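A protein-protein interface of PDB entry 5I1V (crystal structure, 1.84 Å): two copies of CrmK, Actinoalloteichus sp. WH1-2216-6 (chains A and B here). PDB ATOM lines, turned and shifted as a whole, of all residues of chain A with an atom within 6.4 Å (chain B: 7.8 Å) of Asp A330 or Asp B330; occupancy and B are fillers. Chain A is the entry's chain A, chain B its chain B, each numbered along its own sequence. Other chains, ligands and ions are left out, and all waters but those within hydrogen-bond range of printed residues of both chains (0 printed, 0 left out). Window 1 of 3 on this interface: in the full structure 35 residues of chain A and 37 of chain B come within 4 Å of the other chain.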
ATOM      1  N   HIS A  64      -4.375  11.018  17.305  1.00  0.00           N
ATOM      2  CA  HIS A  64      -3.003  10.696  16.933  1.00  0.00           C
ATOM      3  C   HIS A  64      -2.215   9.872  17.886  1.00  0.00           C
ATOM      4  O   HIS A  64      -1.015   9.648  17.648  1.00  0.00           O
ATOM      5  CB  HIS A  64      -2.262  11.989  16.569  1.00  0.00           C
ATOM      6  CG  HIS A  64      -2.435  12.280  15.142  1.00  0.00           C
ATOM      7  ND1 HIS A  64      -1.529  11.841  14.199  1.00  0.00           N
ATOM      8  CD2 HIS A  64      -3.471  12.807  14.461  1.00  0.00           C
ATOM      9  CE1 HIS A  64      -1.997  12.114  12.991  1.00  0.00           C
ATOM     10  NE2 HIS A  64      -3.176  12.686  13.128  1.00  0.00           N
ATOM     11  N   ARG A 109      -3.798  28.071  10.543  1.00  0.00           N
ATOM     12  CA  ARG A 109      -4.405  28.816   9.465  1.00  0.00           C
ATOM     13  C   ARG A 109      -5.254  29.927  10.017  1.00  0.00           C
ATOM     14  O   ARG A 109      -5.192  31.025   9.510  1.00  0.00           O
ATOM     15  CB  ARG A 109      -5.276  27.925   8.577  1.00  0.00           C
ATOM     16  CG  ARG A 109      -4.484  27.168   7.537  1.00  0.00           C
ATOM     17  CD  ARG A 109      -5.447  26.704   6.461  1.00  0.00           C
ATOM     18  NE  ARG A 109      -5.977  25.427   6.851  1.00  0.00           N
ATOM     19  CZ  ARG A 109      -5.542  24.262   6.376  1.00  0.00           C
ATOM     20  NH1 ARG A 109      -4.578  24.206   5.450  1.00  0.00           N
ATOM     21  NH2 ARG A 109      -6.091  23.137   6.824  1.00  0.00           N
ATOM     22  N   MET A 125      -0.815  17.692  10.537  1.00  0.00           N
ATOM     23  CA  MET A 125      -2.022  18.464  10.267  1.00  0.00           C
ATOM     24  C   MET A 125      -3.206  18.103  11.112  1.00  0.00           C
ATOM     25  O   MET A 125      -3.940  18.999  11.557  1.00  0.00           O
ATOM     26  CB  MET A 125      -2.425  18.297   8.801  1.00  0.00           C
ATOM     27  CG  MET A 125      -1.529  19.092   7.870  1.00  0.00           C
ATOM     28  SD  MET A 125      -1.602  20.874   8.210  1.00  0.00           S
ATOM     29  CE  MET A 125      -3.340  21.130   7.752  1.00  0.00           C
ATOM     30  N   GLY A 126      -3.372  16.798  11.355  1.00  0.00           N
ATOM     31  CA  GLY A 126      -4.528  16.295  12.050  1.00  0.00           C
ATOM     32  C   GLY A 126      -4.386  16.121  13.565  1.00  0.00           C
ATOM     33  O   GLY A 126      -5.291  15.602  14.197  1.00  0.00           O
ATOM     34  N   GLN A 324       3.370  24.243   5.705  1.00  0.00           N
ATOM     35  CA  GLN A 324       2.462  23.320   5.048  1.00  0.00           C
ATOM     36  C   GLN A 324       3.254  22.374   4.106  1.00  0.00           C
ATOM     37  O   GLN A 324       2.875  21.218   3.923  1.00  0.00           O
ATOM     38  CB  GLN A 324       1.370  24.079   4.291  1.00  0.00           C
ATOM     39  CG  GLN A 324       0.329  24.727   5.237  1.00  0.00           C
ATOM     40  CD  GLN A 324      -0.663  25.592   4.519  1.00  0.00           C
ATOM     41  OE1 GLN A 324      -0.461  25.931   3.382  1.00  0.00           O
ATOM     42  NE2 GLN A 324      -1.716  26.023   5.220  1.00  0.00           N
ATOM     43  N   ILE A 328       2.704  16.852   7.605  1.00  0.00           N
ATOM     44  CA  ILE A 328       2.199  15.537   7.254  1.00  0.00           C
ATOM     45  C   ILE A 328       0.675  15.580   7.048  1.00  0.00           C
ATOM     46  O   ILE A 328      -0.108  16.034   7.928  1.00  0.00           O
ATOM     47  CB  ILE A 328       2.649  14.451   8.278  1.00  0.00           C
ATOM     48  CG1 ILE A 328       4.109  14.073   8.004  1.00  0.00           C
ATOM     49  CG2 ILE A 328       1.807  13.181   8.172  1.00  0.00           C
ATOM     50  CD1 ILE A 328       5.076  14.911   8.781  1.00  0.00           C
ATOM     51  N   PRO A 329       0.243  15.141   5.874  1.00  0.00           N
ATOM     52  CA  PRO A 329      -1.172  15.161   5.532  1.00  0.00           C
ATOM     53  C   PRO A 329      -2.003  14.279   6.429  1.00  0.00           C
ATOM     54  O   PRO A 329      -1.558  13.204   6.854  1.00  0.00           O
ATOM     55  CB  PRO A 329      -1.226  14.587   4.112  1.00  0.00           C
ATOM     56  CG  PRO A 329       0.171  14.522   3.612  1.00  0.00           C
ATOM     57  CD  PRO A 329       1.107  14.648   4.766  1.00  0.00           C
ATOM     58  N   ASP A 330      -3.231  14.713   6.626  1.00  0.00           N
ATOM     59  CA  ASP A 330      -4.244  13.988   7.386  1.00  0.00           C
ATOM     60  C   ASP A 330      -5.114  13.090   6.478  1.00  0.00           C
ATOM     61  O   ASP A 330      -6.010  12.419   6.962  1.00  0.00           O
ATOM     62  CB  ASP A 330      -5.127  14.996   8.155  1.00  0.00           C
ATOM     63  CG  ASP A 330      -5.766  16.053   7.237  1.00  0.00           C
ATOM     64  OD1 ASP A 330      -5.143  16.462   6.216  1.00  0.00           O
ATOM     65  OD2 ASP A 330      -6.891  16.493   7.556  1.00  0.00           O
ATOM     66  N   VAL A 331      -4.838  13.076   5.169  1.00  0.00           N
ATOM     67  CA  VAL A 331      -5.561  12.221   4.218  1.00  0.00           C
ATOM     68  C   VAL A 331      -4.568  11.636   3.234  1.00  0.00           C
ATOM     69  O   VAL A 331      -3.384  11.977   3.254  1.00  0.00           O
ATOM     70  CB  VAL A 331      -6.627  12.991   3.404  1.00  0.00           C
ATOM     71  CG1 VAL A 331      -7.636  13.660   4.330  1.00  0.00           C
ATOM     72  CG2 VAL A 331      -5.957  13.990   2.478  1.00  0.00           C
ATOM     73  N   GLY A 332      -5.077  10.817   2.335  1.00  0.00           N
ATOM     74  CA  GLY A 332      -4.260  10.136   1.349  1.00  0.00           C
ATOM     75  C   GLY A 332      -3.737   8.850   1.942  1.00  0.00           C
ATOM     76  O   GLY A 332      -3.895   8.594   3.151  1.00  0.00           O
ATOM     77  N   ALA A 335      -1.846   8.437   5.304  1.00  0.00           N
ATOM     78  CA  ALA A 335      -2.492   8.897   6.546  1.00  0.00           C
ATOM     79  C   ALA A 335      -3.606   7.976   7.015  1.00  0.00           C
ATOM     80  O   ALA A 335      -3.863   7.887   8.218  1.00  0.00           O
ATOM     81  CB  ALA A 335      -3.039  10.287   6.320  1.00  0.00           C
ATOM     82  N   ILE A 336      -4.260   7.311   6.061  1.00  0.00           N
ATOM     83  CA  ILE A 336      -5.519   6.619   6.288  1.00  0.00           C
ATOM     84  C   ILE A 336      -5.397   5.120   6.147  1.00  0.00           C
ATOM     85  O   ILE A 336      -4.911   4.633   5.156  1.00  0.00           O
ATOM     86  CB  ILE A 336      -6.594   7.064   5.284  1.00  0.00           C
ATOM     87  CG1 ILE A 336      -6.760   8.590   5.318  1.00  0.00           C
ATOM     88  CG2 ILE A 336      -7.931   6.396   5.621  1.00  0.00           C
ATOM     89  CD1 ILE A 336      -7.387   9.090   6.617  1.00  0.00           C
ATOM     90  N   ASP B  23      -3.378  27.446  -4.876  1.00  0.00           N
ATOM     91  CA  ASP B  23      -2.993  26.086  -5.285  1.00  0.00           C
ATOM     92  C   ASP B  23      -2.087  26.021  -6.536  1.00  0.00           C
ATOM     93  O   ASP B  23      -1.320  25.051  -6.710  1.00  0.00           O
ATOM     94  CB  ASP B  23      -4.255  25.261  -5.537  1.00  0.00           C
ATOM     95  CG  ASP B  23      -3.965  23.817  -5.884  1.00  0.00           C
ATOM     96  OD1 ASP B  23      -3.358  23.130  -5.023  1.00  0.00           O
ATOM     97  OD2 ASP B  23      -4.329  23.381  -7.018  1.00  0.00           O
ATOM     98  N   HIS B  64      -8.563  27.012  -5.460  1.00  0.00           N
ATOM     99  CA  HIS B  64      -8.261  25.894  -6.354  1.00  0.00           C
ATOM    100  C   HIS B  64      -8.398  26.162  -7.840  1.00  0.00           C
ATOM    101  O   HIS B  64      -8.112  25.236  -8.645  1.00  0.00           O
ATOM    102  CB  HIS B  64      -9.020  24.611  -5.966  1.00  0.00           C
ATOM    103  CG  HIS B  64      -8.244  23.821  -4.991  1.00  0.00           C
ATOM    104  ND1 HIS B  64      -7.384  22.815  -5.376  1.00  0.00           N
ATOM    105  CD2 HIS B  64      -8.010  24.024  -3.678  1.00  0.00           C
ATOM    106  CE1 HIS B  64      -6.730  22.365  -4.320  1.00  0.00           C
ATOM    107  NE2 HIS B  64      -7.103  23.085  -3.278  1.00  0.00           N
ATOM    108  N   THR B 103     -14.182  24.389   3.174  1.00  0.00           N
ATOM    109  CA  THR B 103     -13.556  23.500   2.228  1.00  0.00           C
ATOM    110  C   THR B 103     -14.245  22.149   2.274  1.00  0.00           C
ATOM    111  O   THR B 103     -14.835  21.795   3.280  1.00  0.00           O
ATOM    112  CB  THR B 103     -12.079  23.319   2.546  1.00  0.00           C
ATOM    113  OG1 THR B 103     -11.954  22.910   3.912  1.00  0.00           O
ATOM    114  CG2 THR B 103     -11.309  24.595   2.364  1.00  0.00           C
ATOM    115  N   GLY B 105     -13.312  19.031   2.416  1.00  0.00           N
ATOM    116  CA  GLY B 105     -12.837  18.052   3.403  1.00  0.00           C
ATOM    117  C   GLY B 105     -13.475  18.227   4.756  1.00  0.00           C
ATOM    118  O   GLY B 105     -13.906  17.257   5.381  1.00  0.00           O
ATOM    119  N   GLN B 106     -13.507  19.476   5.195  1.00  0.00           N
ATOM    120  CA  GLN B 106     -14.099  19.914   6.456  1.00  0.00           C
ATOM    121  C   GLN B 106     -15.617  19.737   6.438  1.00  0.00           C
ATOM    122  O   GLN B 106     -16.193  19.229   7.392  1.00  0.00           O
ATOM    123  CB  GLN B 106     -13.691  21.381   6.721  1.00  0.00           C
ATOM    124  CG  GLN B 106     -14.665  22.242   7.513  1.00  0.00           C
ATOM    125  CD  GLN B 106     -14.607  23.745   7.169  1.00  0.00           C
ATOM    126  OE1 GLN B 106     -13.842  24.212   6.292  1.00  0.00           O
ATOM    127  NE2 GLN B 106     -15.407  24.524   7.899  1.00  0.00           N
ATOM    128  N   ARG B 109     -16.459  16.052   6.933  1.00  0.00           N
ATOM    129  CA  ARG B 109     -16.143  15.536   8.277  1.00  0.00           C
ATOM    130  C   ARG B 109     -17.272  15.980   9.217  1.00  0.00           C
ATOM    131  O   ARG B 109     -17.781  15.199  10.015  1.00  0.00           O
ATOM    132  CB  ARG B 109     -14.834  16.093   8.815  1.00  0.00           C
ATOM    133  CG  ARG B 109     -13.573  15.609   8.159  1.00  0.00           C
ATOM    134  CD  ARG B 109     -12.421  16.233   8.928  1.00  0.00           C
ATOM    135  NE  ARG B 109     -11.193  15.551   8.568  1.00  0.00           N
ATOM    136  CZ  ARG B 109     -10.276  16.024   7.728  1.00  0.00           C
ATOM    137  NH1 ARG B 109     -10.430  17.221   7.145  1.00  0.00           N
ATOM    138  NH2 ARG B 109      -9.198  15.286   7.456  1.00  0.00           N
ATOM    139  N   CYS B 124     -11.031  16.358  -3.415  1.00  0.00           N
ATOM    140  CA  CYS B 124      -9.833  17.106  -3.001  1.00  0.00           C
ATOM    141  C   CYS B 124     -10.099  17.970  -1.741  1.00  0.00           C
ATOM    142  O   CYS B 124     -11.070  18.703  -1.675  1.00  0.00           O
ATOM    143  CB  CYS B 124      -9.311  17.915  -4.189  1.00  0.00           C
ATOM    144  SG  CYS B 124      -8.938  16.995  -5.749  1.00  0.00           S
ATOM    145  N   MET B 125      -9.227  17.880  -0.744  1.00  0.00           N
ATOM    146  CA  MET B 125      -9.543  18.373   0.596  1.00  0.00           C
ATOM    147  C   MET B 125      -9.632  19.884   0.740  1.00  0.00           C
ATOM    148  O   MET B 125     -10.501  20.352   1.479  1.00  0.00           O
ATOM    149  CB  MET B 125      -8.530  17.838   1.598  1.00  0.00           C
ATOM    150  CG  MET B 125      -8.657  16.325   1.783  1.00  0.00           C
ATOM    151  SD  MET B 125     -10.247  15.776   2.475  1.00  0.00           S
ATOM    152  CE  MET B 125     -10.014  16.407   4.142  1.00  0.00           C
ATOM    153  N   GLY B 126      -8.753  20.641   0.068  1.00  0.00           N
ATOM    154  CA  GLY B 126      -8.753  22.103   0.178  1.00  0.00           C
ATOM    155  C   GLY B 126      -9.674  22.886  -0.781  1.00  0.00           C
ATOM    156  O   GLY B 126      -9.689  24.132  -0.738  1.00  0.00           O
ATOM    157  N   VAL B 127     -10.513  22.191  -1.552  1.00  0.00           N
ATOM    158  CA  VAL B 127     -11.359  22.856  -2.544  1.00  0.00           C
ATOM    159  C   VAL B 127     -12.437  23.633  -1.780  1.00  0.00           C
ATOM    160  O   VAL B 127     -13.042  23.106  -0.840  1.00  0.00           O
ATOM    161  CB  VAL B 127     -11.978  21.822  -3.456  1.00  0.00           C
ATOM    162  CG1 VAL B 127     -13.077  22.391  -4.320  1.00  0.00           C
ATOM    163  CG2 VAL B 127     -10.888  21.174  -4.308  1.00  0.00           C
ATOM    164  N   GLN B 324     -11.386   9.620   2.439  1.00  0.00           N
ATOM    165  CA  GLN B 324     -10.125  10.290   2.814  1.00  0.00           C
ATOM    166  C   GLN B 324      -8.931   9.588   2.218  1.00  0.00           C
ATOM    167  O   GLN B 324      -7.911  10.204   1.958  1.00  0.00           O
ATOM    168  CB  GLN B 324      -9.981  10.457   4.330  1.00  0.00           C
ATOM    169  CG  GLN B 324     -11.070  11.348   4.866  1.00  0.00           C
ATOM    170  CD  GLN B 324     -11.087  11.472   6.361  1.00  0.00           C
ATOM    171  OE1 GLN B 324     -10.693  10.551   7.086  1.00  0.00           O
ATOM    172  NE2 GLN B 324     -11.558  12.603   6.836  1.00  0.00           N
ATOM    173  N   LEU B 325      -9.035   8.292   2.019  1.00  0.00           N
ATOM    174  CA  LEU B 325      -7.888   7.545   1.512  1.00  0.00           C
ATOM    175  C   LEU B 325      -7.575   7.952   0.081  1.00  0.00           C
ATOM    176  O   LEU B 325      -6.427   8.069  -0.311  1.00  0.00           O
ATOM    177  CB  LEU B 325      -8.189   6.061   1.534  1.00  0.00           C
ATOM    178  CG  LEU B 325      -7.115   5.172   0.897  1.00  0.00           C
ATOM    179  CD1 LEU B 325      -5.898   5.047   1.799  1.00  0.00           C
ATOM    180  CD2 LEU B 325      -7.775   3.843   0.652  1.00  0.00           C
ATOM    181  N   ALA B 327      -8.648  10.927  -1.204  1.00  0.00           N
ATOM    182  CA  ALA B 327      -8.578  12.378  -1.360  1.00  0.00           C
ATOM    183  C   ALA B 327      -7.167  12.892  -1.640  1.00  0.00           C
ATOM    184  O   ALA B 327      -6.173  12.267  -1.280  1.00  0.00           O
ATOM    185  CB  ALA B 327      -9.164  13.103  -0.139  1.00  0.00           C
ATOM    186  N   ILE B 328      -7.096  14.035  -2.301  1.00  0.00           N
ATOM    187  CA  ILE B 328      -5.836  14.720  -2.500  1.00  0.00           C
ATOM    188  C   ILE B 328      -5.557  15.660  -1.341  1.00  0.00           C
ATOM    189  O   ILE B 328      -6.427  16.496  -0.997  1.00  0.00           O
ATOM    190  CB  ILE B 328      -5.811  15.477  -3.840  1.00  0.00           C
ATOM    191  CG1 ILE B 328      -5.601  14.469  -4.968  1.00  0.00           C
ATOM    192  CG2 ILE B 328      -4.666  16.491  -3.899  1.00  0.00           C
ATOM    193  CD1 ILE B 328      -6.799  14.249  -5.808  1.00  0.00           C
ATOM    194  N   PRO B 329      -4.362  15.514  -0.719  1.00  0.00           N
ATOM    195  CA  PRO B 329      -3.930  16.395   0.381  1.00  0.00           C
ATOM    196  C   PRO B 329      -3.871  17.871  -0.010  1.00  0.00           C
ATOM    197  O   PRO B 329      -3.478  18.214  -1.124  1.00  0.00           O
ATOM    198  CB  PRO B 329      -2.508  15.909   0.707  1.00  0.00           C
ATOM    199  CG  PRO B 329      -2.408  14.529   0.161  1.00  0.00           C
ATOM    200  CD  PRO B 329      -3.400  14.405  -0.955  1.00  0.00           C
ATOM    201  N   ASP B 330      -4.239  18.713   0.940  1.00  0.00           N
ATOM    202  CA  ASP B 330      -4.042  20.156   0.890  1.00  0.00           C
ATOM    203  C   ASP B 330      -2.685  20.668   1.481  1.00  0.00           C
ATOM    204  O   ASP B 330      -2.438  21.887   1.542  1.00  0.00           O
ATOM    205  CB  ASP B 330      -5.215  20.797   1.636  1.00  0.00           C
ATOM    206  CG  ASP B 330      -5.322  20.293   3.083  1.00  0.00           C
ATOM    207  OD1 ASP B 330      -5.281  19.048   3.299  1.00  0.00           O
ATOM    208  OD2 ASP B 330      -5.428  21.132   3.999  1.00  0.00           O
ATOM    209  N   VAL B 331      -1.824  19.752   1.937  1.00  0.00           N
ATOM    210  CA  VAL B 331      -0.470  20.096   2.409  1.00  0.00           C
ATOM    211  C   VAL B 331       0.502  19.041   1.903  1.00  0.00           C
ATOM    212  O   VAL B 331       0.058  18.018   1.378  1.00  0.00           O
ATOM    213  CB  VAL B 331      -0.373  20.157   3.938  1.00  0.00           C
ATOM    214  CG1 VAL B 331      -1.199  21.329   4.462  1.00  0.00           C
ATOM    215  CG2 VAL B 331      -0.840  18.867   4.553  1.00  0.00           C
ATOM    216  N   GLY B 332       1.797  19.262   2.127  1.00  0.00           N
ATOM    217  CA  GLY B 332       2.850  18.372   1.645  1.00  0.00           C
ATOM    218  C   GLY B 332       3.347  18.780   0.254  1.00  0.00           C
ATOM    219  O   GLY B 332       2.769  19.672  -0.382  1.00  0.00           O
ATOM    220  N   PRO B 333       4.400  18.117  -0.241  1.00  0.00           N
ATOM    221  CA  PRO B 333       5.011  18.405  -1.545  1.00  0.00           C
ATOM    222  C   PRO B 333       4.106  18.291  -2.770  1.00  0.00           C
ATOM    223  O   PRO B 333       4.411  18.887  -3.786  1.00  0.00           O
ATOM    224  CB  PRO B 333       6.174  17.397  -1.624  1.00  0.00           C
ATOM    225  CG  PRO B 333       5.891  16.379  -0.584  1.00  0.00           C
ATOM    226  CD  PRO B 333       5.201  17.133   0.513  1.00  0.00           C
ATOM    227  N   GLY B 334       2.991  17.588  -2.684  1.00  0.00           N
ATOM    228  CA  GLY B 334       2.038  17.550  -3.792  1.00  0.00           C
ATOM    229  C   GLY B 334       1.125  18.759  -3.844  1.00  0.00           C
ATOM    230  O   GLY B 334       0.527  19.050  -4.897  1.00  0.00           O
ATOM    231  N   ALA B 335       0.997  19.469  -2.723  1.00  0.00           N
ATOM    232  CA  ALA B 335       0.025  20.567  -2.650  1.00  0.00           C
ATOM    233  C   ALA B 335       0.649  21.934  -2.689  1.00  0.00           C
ATOM    234  O   ALA B 335       0.045  22.851  -3.223  1.00  0.00           O
ATOM    235  CB  ALA B 335      -0.843  20.451  -1.409  1.00  0.00           C
ATOM    236  N   ILE B 336       1.844  22.082  -2.128  1.00  0.00           N
ATOM    237  CA  ILE B 336       2.358  23.421  -1.800  1.00  0.00           C
ATOM    238  C   ILE B 336       3.526  23.791  -2.683  1.00  0.00           C
ATOM    239  O   ILE B 336       4.456  23.026  -2.849  1.00  0.00           O
ATOM    240  CB  ILE B 336       2.769  23.496  -0.302  1.00  0.00           C
ATOM    241  CG1 ILE B 336       1.591  23.067   0.584  1.00  0.00           C
ATOM    242  CG2 ILE B 336       3.215  24.910   0.060  1.00  0.00           C
ATOM    243  CD1 ILE B 336       0.348  23.937   0.439  1.00  0.00           C
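The backbone NH (N) of Gly A332 lies within hydrogen-bond range of the backbone carbonyl oxygen (O) of Gln B324 (2.9 Å). NH2 of Arg B109 lies within salt-bridge range of OD2 of Asp A330, 2.6 Å away. O of Gln A324 lies within hydrogen-bond range of N of Gly B332. NH1 of Arg A109 is in salt-bridge range of OD2 of Asp B330 (3.5 Å).
N of Met A125 sits at hydrogen-bond distance from O of Ile A328, 3.2 Å away. The guanidinium group (NE) of Arg B109 lies close to the side-chain amide nitrogen (NE2) of Gln B324. O of Met B125 lies within hydrogen-bond range of N of Gly B105, at 3.2 Å. NH1 of Arg A109 sits close to NE2 of Gln A324. The backbone NH (N) of Met B125 is in hydrogen-bond range of the backbone carbonyl oxygen (O) of Ile B328.
Among the printed residues, merely in contact across the chains: Val A331 with Gln B324 (3.4 Å), Met A125 with Val B331 (3.4 Å), Gln A324 with Val B331 (3.4 Å), Gly A332 with Leu B325 (3.4 Å), Ile A336 with Leu B325 (3.5 Å), Val A331 with Met B125 (3.6 Å), Ile A336 with Gln B324 (3.6 Å), Gln A324 with Ile B336 (3.6 Å), Val A331 with Pro B329 (3.8 Å), Pro A329 with Val B331 (3.8 Å), Val A331 with Arg B109 (3.9 Å), Pro A329 with Pro B329 (3.9 Å), Gly A332 with Ala B327 (3.9 Å) and Asp A330 with Asp B330 (3.9 Å).
Of chain B, only Arg B109 (2.6 Å) and Asp B330 (3.9 Å) come within 4 Å of Asp A330. Of chain A, only Arg A109 and Asp A330 come within 4 Å of Asp B330. Of the printed residues of chain B, Gly A332 touches Gln B324 (2.9 Å), Leu B325 (3.4 Å) and Ala B327 (3.9 Å). Of the printed residues of chain A, Val B331 touches Met A125 (3.4 Å), Gln A324 (3.4 Å) and Pro A329 (3.8 Å). Of the printed residues of chain A, Pro B329 touches Pro A329 (3.9 Å) and Val A331 (3.8 Å). His B64 touches none of the printed residues of chain A. Cys B124 touches none of the printed residues of chain A.
Of the 12 printed residues of chain A, 8 touch a printed residue of chain B. Hydrophobic or aromatic side chains of chain A within 4 Å of the printed part of chain B: Met A125, Pro A329, Val A331 and Ile A336. Among the printed residues, Asp or Glu carboxylates within 4 Å of a Lys or Arg side-chain nitrogen of the other chain: Arg A109 with Asp B330 and Asp A330 with Arg B109.
Gln A324 touches Val B331, and with the chains exchanged Val A331 touches Gln B324. Gln A324 touches Ile B336, and with the chains exchanged Ile A336 touches Gln B324. Pro A329 touches Val B331, and with the chains exchanged Val A331 touches Pro B329. Asp B330 touches its own counterpart, Asp A330. Of the 18 pairs that touch across the chains among the printed residues, 14 have their exchanged pair printed and touching as well.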
